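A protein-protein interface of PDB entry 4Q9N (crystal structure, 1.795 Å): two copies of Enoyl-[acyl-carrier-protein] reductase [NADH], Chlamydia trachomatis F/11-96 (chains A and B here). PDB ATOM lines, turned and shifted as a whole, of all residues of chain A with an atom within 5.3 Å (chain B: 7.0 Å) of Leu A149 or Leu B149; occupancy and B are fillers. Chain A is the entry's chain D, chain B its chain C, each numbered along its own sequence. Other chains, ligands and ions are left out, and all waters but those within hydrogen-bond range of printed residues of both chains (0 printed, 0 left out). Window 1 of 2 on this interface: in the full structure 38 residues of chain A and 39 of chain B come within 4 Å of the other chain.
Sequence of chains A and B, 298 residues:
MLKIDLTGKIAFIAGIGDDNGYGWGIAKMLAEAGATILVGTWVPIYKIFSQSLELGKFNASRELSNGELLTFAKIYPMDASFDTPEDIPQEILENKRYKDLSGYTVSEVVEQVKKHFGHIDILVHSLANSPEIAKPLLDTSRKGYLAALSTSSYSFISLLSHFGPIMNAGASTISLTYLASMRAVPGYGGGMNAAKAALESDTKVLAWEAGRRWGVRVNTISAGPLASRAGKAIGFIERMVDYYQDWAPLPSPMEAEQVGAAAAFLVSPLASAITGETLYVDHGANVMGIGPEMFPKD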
ATOM      1  N   GLY A 144     -28.544  14.791 -22.181  1.00  0.00           N
ATOM      2  CA  GLY A 144     -28.292  15.455 -20.915  1.00  0.00           C
ATOM      3  C   GLY A 144     -27.759  16.873 -21.065  1.00  0.00           C
ATOM      4  O   GLY A 144     -28.165  17.773 -20.338  1.00  0.00           O
ATOM      5  N   TYR A 145     -26.836  17.063 -22.001  1.00  0.00           N
ATOM      6  CA  TYR A 145     -26.205  18.363 -22.249  1.00  0.00           C
ATOM      7  C   TYR A 145     -27.265  19.352 -22.714  1.00  0.00           C
ATOM      8  O   TYR A 145     -27.373  20.461 -22.186  1.00  0.00           O
ATOM      9  CB  TYR A 145     -25.145  18.184 -23.336  1.00  0.00           C
ATOM     10  CG  TYR A 145     -24.258  19.372 -23.691  1.00  0.00           C
ATOM     11  CD1 TYR A 145     -23.106  19.652 -22.968  1.00  0.00           C
ATOM     12  CD2 TYR A 145     -24.517  20.135 -24.824  1.00  0.00           C
ATOM     13  CE1 TYR A 145     -22.269  20.718 -23.330  1.00  0.00           C
ATOM     14  CE2 TYR A 145     -23.693  21.182 -25.197  1.00  0.00           C
ATOM     15  CZ  TYR A 145     -22.572  21.470 -24.449  1.00  0.00           C
ATOM     16  OH  TYR A 145     -21.767  22.513 -24.848  1.00  0.00           O
ATOM     17  N   LEU A 146     -28.033  18.953 -23.716  1.00  0.00           N
ATOM     18  CA  LEU A 146     -29.083  19.820 -24.259  1.00  0.00           C
ATOM     19  C   LEU A 146     -30.236  20.079 -23.277  1.00  0.00           C
ATOM     20  O   LEU A 146     -30.858  21.139 -23.317  1.00  0.00           O
ATOM     21  CB  LEU A 146     -29.615  19.262 -25.581  1.00  0.00           C
ATOM     22  CG  LEU A 146     -28.574  19.223 -26.708  1.00  0.00           C
ATOM     23  CD1 LEU A 146     -29.105  18.506 -27.946  1.00  0.00           C
ATOM     24  CD2 LEU A 146     -28.087  20.628 -27.047  1.00  0.00           C
ATOM     25  N   ALA A 147     -30.531  19.118 -22.409  1.00  0.00           N
ATOM     26  CA  ALA A 147     -31.531  19.348 -21.361  1.00  0.00           C
ATOM     27  C   ALA A 147     -31.029  20.428 -20.394  1.00  0.00           C
ATOM     28  O   ALA A 147     -31.789  21.288 -19.945  1.00  0.00           O
ATOM     29  CB  ALA A 147     -31.833  18.049 -20.618  1.00  0.00           C
ATOM     30  N   ALA A 148     -29.740  20.386 -20.078  1.00  0.00           N
ATOM     31  CA  ALA A 148     -29.149  21.392 -19.197  1.00  0.00           C
ATOM     32  C   ALA A 148     -29.269  22.770 -19.826  1.00  0.00           C
ATOM     33  O   ALA A 148     -29.611  23.726 -19.152  1.00  0.00           O
ATOM     34  CB  ALA A 148     -27.684  21.081 -18.913  1.00  0.00           C
ATOM     35  N   LEU A 149     -28.996  22.861 -21.122  1.00  0.00           N
ATOM     36  CA  LEU A 149     -29.091  24.143 -21.806  1.00  0.00           C
ATOM     37  C   LEU A 149     -30.537  24.595 -21.924  1.00  0.00           C
ATOM     38  O   LEU A 149     -30.847  25.774 -21.769  1.00  0.00           O
ATOM     39  CB  LEU A 149     -28.439  24.069 -23.181  1.00  0.00           C
ATOM     40  CG  LEU A 149     -26.908  24.194 -23.097  1.00  0.00           C
ATOM     41  CD1 LEU A 149     -26.257  23.370 -24.186  1.00  0.00           C
ATOM     42  CD2 LEU A 149     -26.453  25.673 -23.155  1.00  0.00           C
ATOM     43  N   SER A 150     -31.423  23.644 -22.178  1.00  0.00           N
ATOM     44  CA  SER A 150     -32.825  23.975 -22.379  1.00  0.00           C
ATOM     45  C   SER A 150     -33.434  24.561 -21.103  1.00  0.00           C
ATOM     46  O   SER A 150     -34.089  25.607 -21.131  1.00  0.00           O
ATOM     47  CB  SER A 150     -33.600  22.729 -22.819  1.00  0.00           C
ATOM     48  OG  SER A 150     -34.949  23.063 -23.121  1.00  0.00           O
ATOM     49  N   THR A 151     -33.221  23.872 -19.988  1.00  0.00           N
ATOM     50  CA  THR A 151     -33.796  24.270 -18.717  1.00  0.00           C
ATOM     51  C   THR A 151     -33.081  25.476 -18.122  1.00  0.00           C
ATOM     52  O   THR A 151     -33.705  26.352 -17.560  1.00  0.00           O
ATOM     53  CB  THR A 151     -33.753  23.116 -17.700  1.00  0.00           C
ATOM     54  OG1 THR A 151     -34.465  21.985 -18.211  1.00  0.00           O
ATOM     55  CG2 THR A 151     -34.349  23.531 -16.365  1.00  0.00           C
ATOM     56  N   SER A 152     -31.760  25.507 -18.227  1.00  0.00           N
ATOM     57  CA  SER A 152     -30.997  26.496 -17.490  1.00  0.00           C
ATOM     58  C   SER A 152     -30.683  27.757 -18.266  1.00  0.00           C
ATOM     59  O   SER A 152     -30.402  28.789 -17.666  1.00  0.00           O
ATOM     60  CB  SER A 152     -29.703  25.869 -16.967  1.00  0.00           C
ATOM     61  OG  SER A 152     -30.001  24.629 -16.349  1.00  0.00           O
ATOM     62  N   SER A 153     -30.706  27.670 -19.592  1.00  0.00           N
ATOM     63  CA  SER A 153     -30.312  28.796 -20.433  1.00  0.00           C
ATOM     64  C   SER A 153     -31.423  29.272 -21.346  1.00  0.00           C
ATOM     65  O   SER A 153     -31.817  30.444 -21.285  1.00  0.00           O
ATOM     66  CB  SER A 153     -29.088  28.435 -21.280  1.00  0.00           C
ATOM     67  OG  SER A 153     -28.062  27.923 -20.452  1.00  0.00           O
ATOM     68  N   TYR A 154     -31.914  28.383 -22.207  1.00  0.00           N
ATOM     69  CA  TYR A 154     -32.927  28.788 -23.166  1.00  0.00           C
ATOM     70  C   TYR A 154     -34.199  29.293 -22.468  1.00  0.00           C
ATOM     71  O   TYR A 154     -34.864  30.190 -22.975  1.00  0.00           O
ATOM     72  CB  TYR A 154     -33.276  27.696 -24.199  1.00  0.00           C
ATOM     73  CG  TYR A 154     -34.223  28.303 -25.195  1.00  0.00           C
ATOM     74  CD1 TYR A 154     -33.748  29.093 -26.237  1.00  0.00           C
ATOM     75  CD2 TYR A 154     -35.597  28.201 -25.022  1.00  0.00           C
ATOM     76  CE1 TYR A 154     -34.629  29.722 -27.121  1.00  0.00           C
ATOM     77  CE2 TYR A 154     -36.480  28.823 -25.891  1.00  0.00           C
ATOM     78  CZ  TYR A 154     -35.989  29.584 -26.938  1.00  0.00           C
ATOM     79  OH  TYR A 154     -36.864  30.193 -27.810  1.00  0.00           O
ATOM     80  N   SER A 155     -34.527  28.711 -21.315  1.00  0.00           N
ATOM     81  CA  SER A 155     -35.686  29.157 -20.540  1.00  0.00           C
ATOM     82  C   SER A 155     -35.662  30.663 -20.267  1.00  0.00           C
ATOM     83  O   SER A 155     -36.711  31.312 -20.244  1.00  0.00           O
ATOM     84  CB  SER A 155     -35.773  28.392 -19.220  1.00  0.00           C
ATOM     85  OG  SER A 155     -34.567  28.536 -18.491  1.00  0.00           O
ATOM     86  N   GLY A 191     -22.912  19.277 -18.337  1.00  0.00           N
ATOM     87  CA  GLY A 191     -23.054  20.433 -19.206  1.00  0.00           C
ATOM     88  C   GLY A 191     -23.491  21.717 -18.511  1.00  0.00           C
ATOM     89  O   GLY A 191     -23.797  22.713 -19.173  1.00  0.00           O
ATOM     90  N   ALA A 194     -21.527  24.723 -19.643  1.00  0.00           N
ATOM     91  CA  ALA A 194     -21.935  25.265 -20.925  1.00  0.00           C
ATOM     92  C   ALA A 194     -23.235  26.041 -20.761  1.00  0.00           C
ATOM     93  O   ALA A 194     -23.407  27.088 -21.375  1.00  0.00           O
ATOM     94  CB  ALA A 194     -22.111  24.164 -21.938  1.00  0.00           C
ATOM     95  N   ALA A 195     -24.131  25.531 -19.922  1.00  0.00           N
ATOM     96  CA  ALA A 195     -25.409  26.200 -19.688  1.00  0.00           C
ATOM     97  C   ALA A 195     -25.167  27.570 -19.073  1.00  0.00           C
ATOM     98  O   ALA A 195     -25.817  28.541 -19.448  1.00  0.00           O
ATOM     99  CB  ALA A 195     -26.310  25.369 -18.779  1.00  0.00           C
ATOM    100  N   ALA A 198     -23.543  29.916 -21.724  1.00  0.00           N
ATOM    101  CA  ALA A 198     -24.600  30.367 -22.626  1.00  0.00           C
ATOM    102  C   ALA A 198     -25.448  31.448 -21.970  1.00  0.00           C
ATOM    103  O   ALA A 198     -25.768  32.446 -22.601  1.00  0.00           O
ATOM    104  CB  ALA A 198     -25.480  29.185 -23.070  1.00  0.00           C
ATOM    105  N   ASN B 129     -23.195  25.100 -37.245  1.00  0.00           N
ATOM    106  CA  ASN B 129     -24.422  25.456 -37.947  1.00  0.00           C
ATOM    107  C   ASN B 129     -25.495  25.865 -36.971  1.00  0.00           C
ATOM    108  O   ASN B 129     -25.603  25.315 -35.874  1.00  0.00           O
ATOM    109  CB  ASN B 129     -24.948  24.317 -38.826  1.00  0.00           C
ATOM    110  CG  ASN B 129     -26.159  24.731 -39.639  1.00  0.00           C
ATOM    111  OD1 ASN B 129     -26.029  25.293 -40.728  1.00  0.00           O
ATOM    112  ND2 ASN B 129     -27.349  24.476 -39.101  1.00  0.00           N
ATOM    113  N   SER B 130     -26.295  26.838 -37.388  1.00  0.00           N
ATOM    114  CA  SER B 130     -27.543  27.129 -36.730  1.00  0.00           C
ATOM    115  C   SER B 130     -28.568  27.323 -37.821  1.00  0.00           C
ATOM    116  O   SER B 130     -28.308  28.020 -38.802  1.00  0.00           O
ATOM    117  CB  SER B 130     -27.443  28.412 -35.903  1.00  0.00           C
ATOM    118  OG  SER B 130     -28.733  28.806 -35.457  1.00  0.00           O
ATOM    119  N   ARG B 142     -36.637  27.473 -29.449  1.00  0.00           N
ATOM    120  CA  ARG B 142     -35.923  26.514 -28.613  1.00  0.00           C
ATOM    121  C   ARG B 142     -35.254  25.456 -29.484  1.00  0.00           C
ATOM    122  O   ARG B 142     -34.094  25.089 -29.268  1.00  0.00           O
ATOM    123  CB  ARG B 142     -36.864  25.847 -27.606  1.00  0.00           C
ATOM    124  CG  ARG B 142     -36.117  25.089 -26.506  1.00  0.00           C
ATOM    125  CD  ARG B 142     -37.077  24.466 -25.516  1.00  0.00           C
ATOM    126  NE  ARG B 142     -37.933  25.429 -24.809  1.00  0.00           N
ATOM    127  CZ  ARG B 142     -37.701  25.849 -23.568  1.00  0.00           C
ATOM    128  NH1 ARG B 142     -36.639  25.397 -22.899  1.00  0.00           N
ATOM    129  NH2 ARG B 142     -38.529  26.705 -22.987  1.00  0.00           N
ATOM    130  N   LYS B 143     -35.992  24.984 -30.482  1.00  0.00           N
ATOM    131  CA  LYS B 143     -35.480  23.976 -31.400  1.00  0.00           C
ATOM    132  C   LYS B 143     -34.242  24.499 -32.135  1.00  0.00           C
ATOM    133  O   LYS B 143     -33.229  23.799 -32.240  1.00  0.00           O
ATOM    134  CB  LYS B 143     -36.573  23.566 -32.393  1.00  0.00           C
ATOM    135  CG  LYS B 143     -36.295  22.276 -33.140  1.00  0.00           C
ATOM    136  CD  LYS B 143     -37.424  21.981 -34.119  1.00  0.00           C
ATOM    137  CE  LYS B 143     -37.244  20.639 -34.819  1.00  0.00           C
ATOM    138  NZ  LYS B 143     -38.405  20.346 -35.721  1.00  0.00           N
ATOM    139  N   GLY B 144     -34.317  25.734 -32.623  1.00  0.00           N
ATOM    140  CA  GLY B 144     -33.185  26.345 -33.312  1.00  0.00           C
ATOM    141  C   GLY B 144     -31.938  26.493 -32.452  1.00  0.00           C
ATOM    142  O   GLY B 144     -30.825  26.150 -32.869  1.00  0.00           O
ATOM    143  N   TYR B 145     -32.130  27.010 -31.244  1.00  0.00           N
ATOM    144  CA  TYR B 145     -31.043  27.254 -30.290  1.00  0.00           C
ATOM    145  C   TYR B 145     -30.371  25.941 -29.913  1.00  0.00           C
ATOM    146  O   TYR B 145     -29.147  25.830 -29.932  1.00  0.00           O
ATOM    147  CB  TYR B 145     -31.645  27.896 -29.052  1.00  0.00           C
ATOM    148  CG  TYR B 145     -30.739  28.308 -27.904  1.00  0.00           C
ATOM    149  CD1 TYR B 145     -30.214  29.596 -27.842  1.00  0.00           C
ATOM    150  CD2 TYR B 145     -30.524  27.457 -26.824  1.00  0.00           C
ATOM    151  CE1 TYR B 145     -29.439  30.008 -26.768  1.00  0.00           C
ATOM    152  CE2 TYR B 145     -29.744  27.860 -25.741  1.00  0.00           C
ATOM    153  CZ  TYR B 145     -29.210  29.143 -25.728  1.00  0.00           C
ATOM    154  OH  TYR B 145     -28.460  29.561 -24.661  1.00  0.00           O
ATOM    155  N   LEU B 146     -31.176  24.939 -29.579  1.00  0.00           N
ATOM    156  CA  LEU B 146     -30.610  23.652 -29.187  1.00  0.00           C
ATOM    157  C   LEU B 146     -29.919  22.965 -30.362  1.00  0.00           C
ATOM    158  O   LEU B 146     -28.921  22.271 -30.175  1.00  0.00           O
ATOM    159  CB  LEU B 146     -31.659  22.751 -28.533  1.00  0.00           C
ATOM    160  CG  LEU B 146     -32.217  23.297 -27.209  1.00  0.00           C
ATOM    161  CD1 LEU B 146     -33.245  22.348 -26.607  1.00  0.00           C
ATOM    162  CD2 LEU B 146     -31.085  23.578 -26.215  1.00  0.00           C
ATOM    163  N   ALA B 147     -30.418  23.183 -31.573  1.00  0.00           N
ATOM    164  CA  ALA B 147     -29.775  22.599 -32.752  1.00  0.00           C
ATOM    165  C   ALA B 147     -28.401  23.217 -32.993  1.00  0.00           C
ATOM    166  O   ALA B 147     -27.437  22.511 -33.332  1.00  0.00           O
ATOM    167  CB  ALA B 147     -30.662  22.757 -33.976  1.00  0.00           C
ATOM    168  N   ALA B 148     -28.302  24.535 -32.818  1.00  0.00           N
ATOM    169  CA  ALA B 148     -27.011  25.203 -32.904  1.00  0.00           C
ATOM    170  C   ALA B 148     -26.051  24.604 -31.878  1.00  0.00           C
ATOM    171  O   ALA B 148     -24.915  24.281 -32.198  1.00  0.00           O
ATOM    172  CB  ALA B 148     -27.163  26.728 -32.678  1.00  0.00           C
ATOM    173  N   LEU B 149     -26.518  24.433 -30.647  1.00  0.00           N
ATOM    174  CA  LEU B 149     -25.671  23.859 -29.609  1.00  0.00           C
ATOM    175  C   LEU B 149     -25.279  22.408 -29.905  1.00  0.00           C
ATOM    176  O   LEU B 149     -24.116  22.011 -29.739  1.00  0.00           O
ATOM    177  CB  LEU B 149     -26.338  23.979 -28.240  1.00  0.00           C
ATOM    178  CG  LEU B 149     -26.112  25.357 -27.601  1.00  0.00           C
ATOM    179  CD1 LEU B 149     -27.307  25.739 -26.762  1.00  0.00           C
ATOM    180  CD2 LEU B 149     -24.821  25.361 -26.774  1.00  0.00           C
ATOM    181  N   SER B 150     -26.250  21.623 -30.358  1.00  0.00           N
ATOM    182  CA  SER B 150     -25.991  20.225 -30.697  1.00  0.00           C
ATOM    183  C   SER B 150     -24.950  20.091 -31.810  1.00  0.00           C
ATOM    184  O   SER B 150     -23.956  19.375 -31.668  1.00  0.00           O
ATOM    185  CB  SER B 150     -27.300  19.538 -31.089  1.00  0.00           C
ATOM    186  OG  SER B 150     -27.095  18.169 -31.367  1.00  0.00           O
ATOM    187  N   THR B 151     -25.165  20.796 -32.914  1.00  0.00           N
ATOM    188  CA  THR B 151     -24.237  20.733 -34.043  1.00  0.00           C
ATOM    189  C   THR B 151     -22.883  21.406 -33.790  1.00  0.00           C
ATOM    190  O   THR B 151     -21.848  20.852 -34.147  1.00  0.00           O
ATOM    191  CB  THR B 151     -24.866  21.340 -35.302  1.00  0.00           C
ATOM    192  OG1 THR B 151     -26.050  20.614 -35.633  1.00  0.00           O
ATOM    193  CG2 THR B 151     -23.907  21.288 -36.469  1.00  0.00           C
ATOM    194  N   SER B 152     -22.890  22.596 -33.183  1.00  0.00           N
ATOM    195  CA  SER B 152     -21.689  23.432 -33.116  1.00  0.00           C
ATOM    196  C   SER B 152     -20.854  23.213 -31.864  1.00  0.00           C
ATOM    197  O   SER B 152     -19.649  23.519 -31.845  1.00  0.00           O
ATOM    198  CB  SER B 152     -22.068  24.917 -33.215  1.00  0.00           C
ATOM    199  OG  SER B 152     -22.867  25.160 -34.354  1.00  0.00           O
ATOM    200  N   SER B 153     -21.484  22.699 -30.813  1.00  0.00           N
ATOM    201  CA  SER B 153     -20.798  22.567 -29.536  1.00  0.00           C
ATOM    202  C   SER B 153     -20.763  21.142 -28.974  1.00  0.00           C
ATOM    203  O   SER B 153     -19.681  20.624 -28.669  1.00  0.00           O
ATOM    204  CB  SER B 153     -21.342  23.571 -28.511  1.00  0.00           C
ATOM    205  OG  SER B 153     -22.263  22.975 -27.621  1.00  0.00           O
ATOM    206  N   TYR B 154     -21.918  20.499 -28.826  1.00  0.00           N
ATOM    207  CA  TYR B 154     -21.878  19.122 -28.327  1.00  0.00           C
ATOM    208  C   TYR B 154     -21.087  18.195 -29.248  1.00  0.00           C
ATOM    209  O   TYR B 154     -20.383  17.306 -28.768  1.00  0.00           O
ATOM    210  CB  TYR B 154     -23.256  18.525 -28.022  1.00  0.00           C
ATOM    211  CG  TYR B 154     -23.085  17.194 -27.319  1.00  0.00           C
ATOM    212  CD1 TYR B 154     -22.830  17.142 -25.954  1.00  0.00           C
ATOM    213  CD2 TYR B 154     -23.134  15.995 -28.026  1.00  0.00           C
ATOM    214  CE1 TYR B 154     -22.643  15.926 -25.307  1.00  0.00           C
ATOM    215  CE2 TYR B 154     -22.953  14.783 -27.390  1.00  0.00           C
ATOM    216  CZ  TYR B 154     -22.704  14.753 -26.033  1.00  0.00           C
ATOM    217  OH  TYR B 154     -22.513  13.541 -25.401  1.00  0.00           O
ATOM    218  N   SER B 155     -21.168  18.432 -30.556  1.00  0.00           N
ATOM    219  CA  SER B 155     -20.425  17.632 -31.540  1.00  0.00           C
ATOM    220  C   SER B 155     -18.950  17.479 -31.158  1.00  0.00           C
ATOM    221  O   SER B 155     -18.336  16.446 -31.431  1.00  0.00           O
ATOM    222  CB  SER B 155     -20.527  18.260 -32.932  1.00  0.00           C
ATOM    223  OG  SER B 155     -20.140  19.629 -32.895  1.00  0.00           O
ATOM    224  N   PHE B 156     -18.389  18.498 -30.511  1.00  0.00           N
ATOM    225  CA  PHE B 156     -16.990  18.403 -30.104  1.00  0.00           C
ATOM    226  C   PHE B 156     -16.820  17.431 -28.944  1.00  0.00           C
ATOM    227  O   PHE B 156     -15.878  16.647 -28.920  1.00  0.00           O
ATOM    228  CB  PHE B 156     -16.369  19.754 -29.728  1.00  0.00           C
ATOM    229  CG  PHE B 156     -14.935  19.622 -29.293  1.00  0.00           C
ATOM    230  CD1 PHE B 156     -13.930  19.504 -30.235  1.00  0.00           C
ATOM    231  CD2 PHE B 156     -14.608  19.535 -27.953  1.00  0.00           C
ATOM    232  CE1 PHE B 156     -12.602  19.327 -29.849  1.00  0.00           C
ATOM    233  CE2 PHE B 156     -13.272  19.366 -27.557  1.00  0.00           C
ATOM    234  CZ  PHE B 156     -12.284  19.267 -28.506  1.00  0.00           C
ATOM    235  N   GLY B 190     -29.464  33.066 -33.878  1.00  0.00           N
ATOM    236  CA  GLY B 190     -29.803  31.654 -33.909  1.00  0.00           C
ATOM    237  C   GLY B 190     -29.158  30.886 -32.773  1.00  0.00           C
ATOM    238  O   GLY B 190     -29.095  29.653 -32.804  1.00  0.00           O
ATOM    239  N   GLY B 191     -28.687  31.619 -31.767  1.00  0.00           N
ATOM    240  CA  GLY B 191     -27.969  31.018 -30.660  1.00  0.00           C
ATOM    241  C   GLY B 191     -26.511  30.683 -30.952  1.00  0.00           C
ATOM    242  O   GLY B 191     -25.870  29.981 -30.166  1.00  0.00           O
ATOM    243  N   MET B 192     -25.972  31.149 -32.078  1.00  0.00           N
ATOM    244  CA  MET B 192     -24.551  30.893 -32.350  1.00  0.00           C
ATOM    245  C   MET B 192     -23.663  31.485 -31.263  1.00  0.00           C
ATOM    246  O   MET B 192     -22.598  30.946 -30.968  1.00  0.00           O
ATOM    247  CB  MET B 192     -24.107  31.419 -33.719  1.00  0.00           C
ATOM    248  CG  MET B 192     -24.508  30.554 -34.887  1.00  0.00           C
ATOM    249  SD  MET B 192     -24.065  28.811 -34.680  1.00  0.00           S
ATOM    250  CE  MET B 192     -22.276  28.916 -34.463  1.00  0.00           C
ATOM    251  N   ALA B 194     -24.278  31.551 -28.065  1.00  0.00           N
ATOM    252  CA  ALA B 194     -24.323  30.564 -26.995  1.00  0.00           C
ATOM    253  C   ALA B 194     -23.525  29.324 -27.370  1.00  0.00           C
ATOM    254  O   ALA B 194     -22.849  28.735 -26.526  1.00  0.00           O
ATOM    255  CB  ALA B 194     -25.776  30.199 -26.680  1.00  0.00           C
ATOM    256  N   ALA B 195     -23.602  28.932 -28.640  1.00  0.00           N
ATOM    257  CA  ALA B 195     -22.867  27.770 -29.110  1.00  0.00           C
ATOM    258  C   ALA B 195     -21.365  28.005 -28.993  1.00  0.00           C
ATOM    259  O   ALA B 195     -20.625  27.099 -28.615  1.00  0.00           O
ATOM    260  CB  ALA B 195     -23.257  27.412 -30.547  1.00  0.00           C
ATOM    261  N   LYS B 196     -20.907  29.219 -29.278  1.00  0.00           N
ATOM    262  CA  LYS B 196     -19.469  29.469 -29.150  1.00  0.00           C
ATOM    263  C   LYS B 196     -19.054  29.672 -27.695  1.00  0.00           C
ATOM    264  O   LYS B 196     -17.953  29.283 -27.316  1.00  0.00           O
ATOM    265  CB  LYS B 196     -19.005  30.640 -30.024  1.00  0.00           C
ATOM    266  CG  LYS B 196     -19.149  30.408 -31.524  1.00  0.00           C
ATOM    267  CD  LYS B 196     -18.544  29.082 -31.971  1.00  0.00           C
ATOM    268  CE  LYS B 196     -18.379  29.046 -33.489  1.00  0.00           C
ATOM    269  NZ  LYS B 196     -17.651  27.833 -33.966  1.00  0.00           N
ATOM    270  N   ALA B 197     -19.915  30.286 -26.883  1.00  0.00           N
ATOM    271  CA  ALA B 197     -19.645  30.393 -25.453  1.00  0.00           C
ATOM    272  C   ALA B 197     -19.490  28.992 -24.854  1.00  0.00           C
ATOM    273  O   ALA B 197     -18.566  28.717 -24.083  1.00  0.00           O
ATOM    274  CB  ALA B 197     -20.766  31.138 -24.755  1.00  0.00           C
ATOM    275  N   ALA B 198     -20.414  28.111 -25.216  1.00  0.00           N
ATOM    276  CA  ALA B 198     -20.354  26.721 -24.781  1.00  0.00           C
ATOM    277  C   ALA B 198     -19.061  26.062 -25.258  1.00  0.00           C
ATOM    278  O   ALA B 198     -18.365  25.431 -24.476  1.00  0.00           O
ATOM    279  CB  ALA B 198     -21.559  25.961 -25.271  1.00  0.00           C
ATOM    280  N   LEU B 199     -18.734  26.233 -26.536  1.00  0.00           N
ATOM    281  CA  LEU B 199     -17.498  25.673 -27.082  1.00  0.00           C
ATOM    282  C   LEU B 199     -16.263  26.129 -26.299  1.00  0.00           C
ATOM    283  O   LEU B 199     -15.371  25.328 -26.001  1.00  0.00           O
ATOM    284  CB  LEU B 199     -17.365  26.030 -28.561  1.00  0.00           C
ATOM    285  CG  LEU B 199     -16.227  25.353 -29.326  1.00  0.00           C
ATOM    286  CD1 LEU B 199     -16.491  23.850 -29.458  1.00  0.00           C
ATOM    287  CD2 LEU B 199     -16.060  25.991 -30.693  1.00  0.00           C
ATOM    288  N   ASP B 202     -16.318  24.632 -22.738  1.00  0.00           N
ATOM    289  CA  ASP B 202     -16.045  23.192 -22.778  1.00  0.00           C
ATOM    290  C   ASP B 202     -14.547  22.981 -23.016  1.00  0.00           C
ATOM    291  O   ASP B 202     -13.965  22.036 -22.495  1.00  0.00           O
ATOM    292  CB  ASP B 202     -16.865  22.469 -23.862  1.00  0.00           C
ATOM    293  CG  ASP B 202     -18.382  22.538 -23.620  1.00  0.00           C
ATOM    294  OD1 ASP B 202     -18.806  22.779 -22.468  1.00  0.00           O
ATOM    295  OD2 ASP B 202     -19.149  22.341 -24.596  1.00  0.00           O
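The backbone NH of Arg B142 lies within hydrogen-bond range of the side-chain hydroxyl of Tyr A154, at 3.2 Å. The guanidinium group of Arg B142 lies within hydrogen-bond range of the side-chain hydroxyl of Ser A150. OG of Ser B153 lies within hydrogen-bond range of OH of Tyr A145 (2.9 Å). The side-chain carboxylate (OD2) of Asp B202 lies within hydrogen-bond range of the side-chain hydroxyl (OH) of Tyr A145, 2.6 Å away.
O of Leu A149 lies within hydrogen-bond range of N of Tyr A154, 2.9 Å away. The side-chain hydroxyl (OG) of Ser A153 is in hydrogen-bond range of the backbone carbonyl oxygen (O) of Ala A195. The backbone NH (N) of Tyr B154 sits at hydrogen-bond distance from the backbone carbonyl oxygen (O) of Leu B149 (2.8 Å). N of Ser B155 is in hydrogen-bond range of O of Ser B150, at 3.1 Å. O of Leu B149 is in hydrogen-bond range of OG of Ser B153 (3.0 Å). The backbone carbonyl oxygen of Ser A150 sits at hydrogen-bond distance from the backbone NH of Ser A155 (3.1 Å).
Among the printed residues, pairs that only touch across the chains: Ala A198 with Tyr B145 (3.4 Å), Tyr A145 with Ala B198 (3.5 Å), Tyr A145 with Tyr B154 (3.5 Å), Tyr A154 with Tyr B145 (3.5 Å), Leu A149 with Leu B149 (3.6 Å), Ser A153 with Tyr B145 (3.6 Å), Ala A194 with Asp B202 (3.6 Å), Leu A146 with Leu B146 (3.6 Å), Ala A198 with Ala B194 (3.8 Å), Leu A146 with Ser B150 (3.8 Å), Ser A150 with Leu B146 (3.8 Å), Ala A194 with Ala B198 (3.8 Å) and Leu A146 with Leu B149 (3.96 Å).
Of chain B, only Leu B149 (3.6 Å) comes within 4 Å of Leu A149. Gly A191 touches none of the printed residues of chain B. Of the printed residues of chain B, Ala A194 touches Ala B198 (3.8 Å) and Asp B202 (3.6 Å). Leu B149 touches two residues of chain A. Of the printed residues of chain A, Ser B150 touches Leu A146 (3.8 Å). Ser B152 touches none of the printed residues of chain A. The nearest residue of chain A that does not touch Leu B149 is Tyr A145 (4.6 Å). The nearest printed residue of chain A that does not touch Ser B150 is Tyr A145 (5.8 Å).
Of the 16 printed residues of chain A, 8 touch a printed residue of chain B. Hydrophobic or aromatic side chains of chain B within 4 Å of the printed part of chain A: Tyr B145, Leu B146, Leu B149, Tyr B154, Ala B194 and Ala B198. Among the printed residues, no Asp or Glu carboxylate lies within 4 Å of a Lys or Arg side-chain nitrogen of the other chain.
Tyr A145 touches Tyr B154, and with the chains exchanged Tyr A154 touches Tyr B145. Leu A146 touches its own counterpart, Leu B146. Leu A146 touches Ser B150, and with the chains exchanged Ser A150 touches Leu B146. Leu B149 touches its own counterpart, Leu A149.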
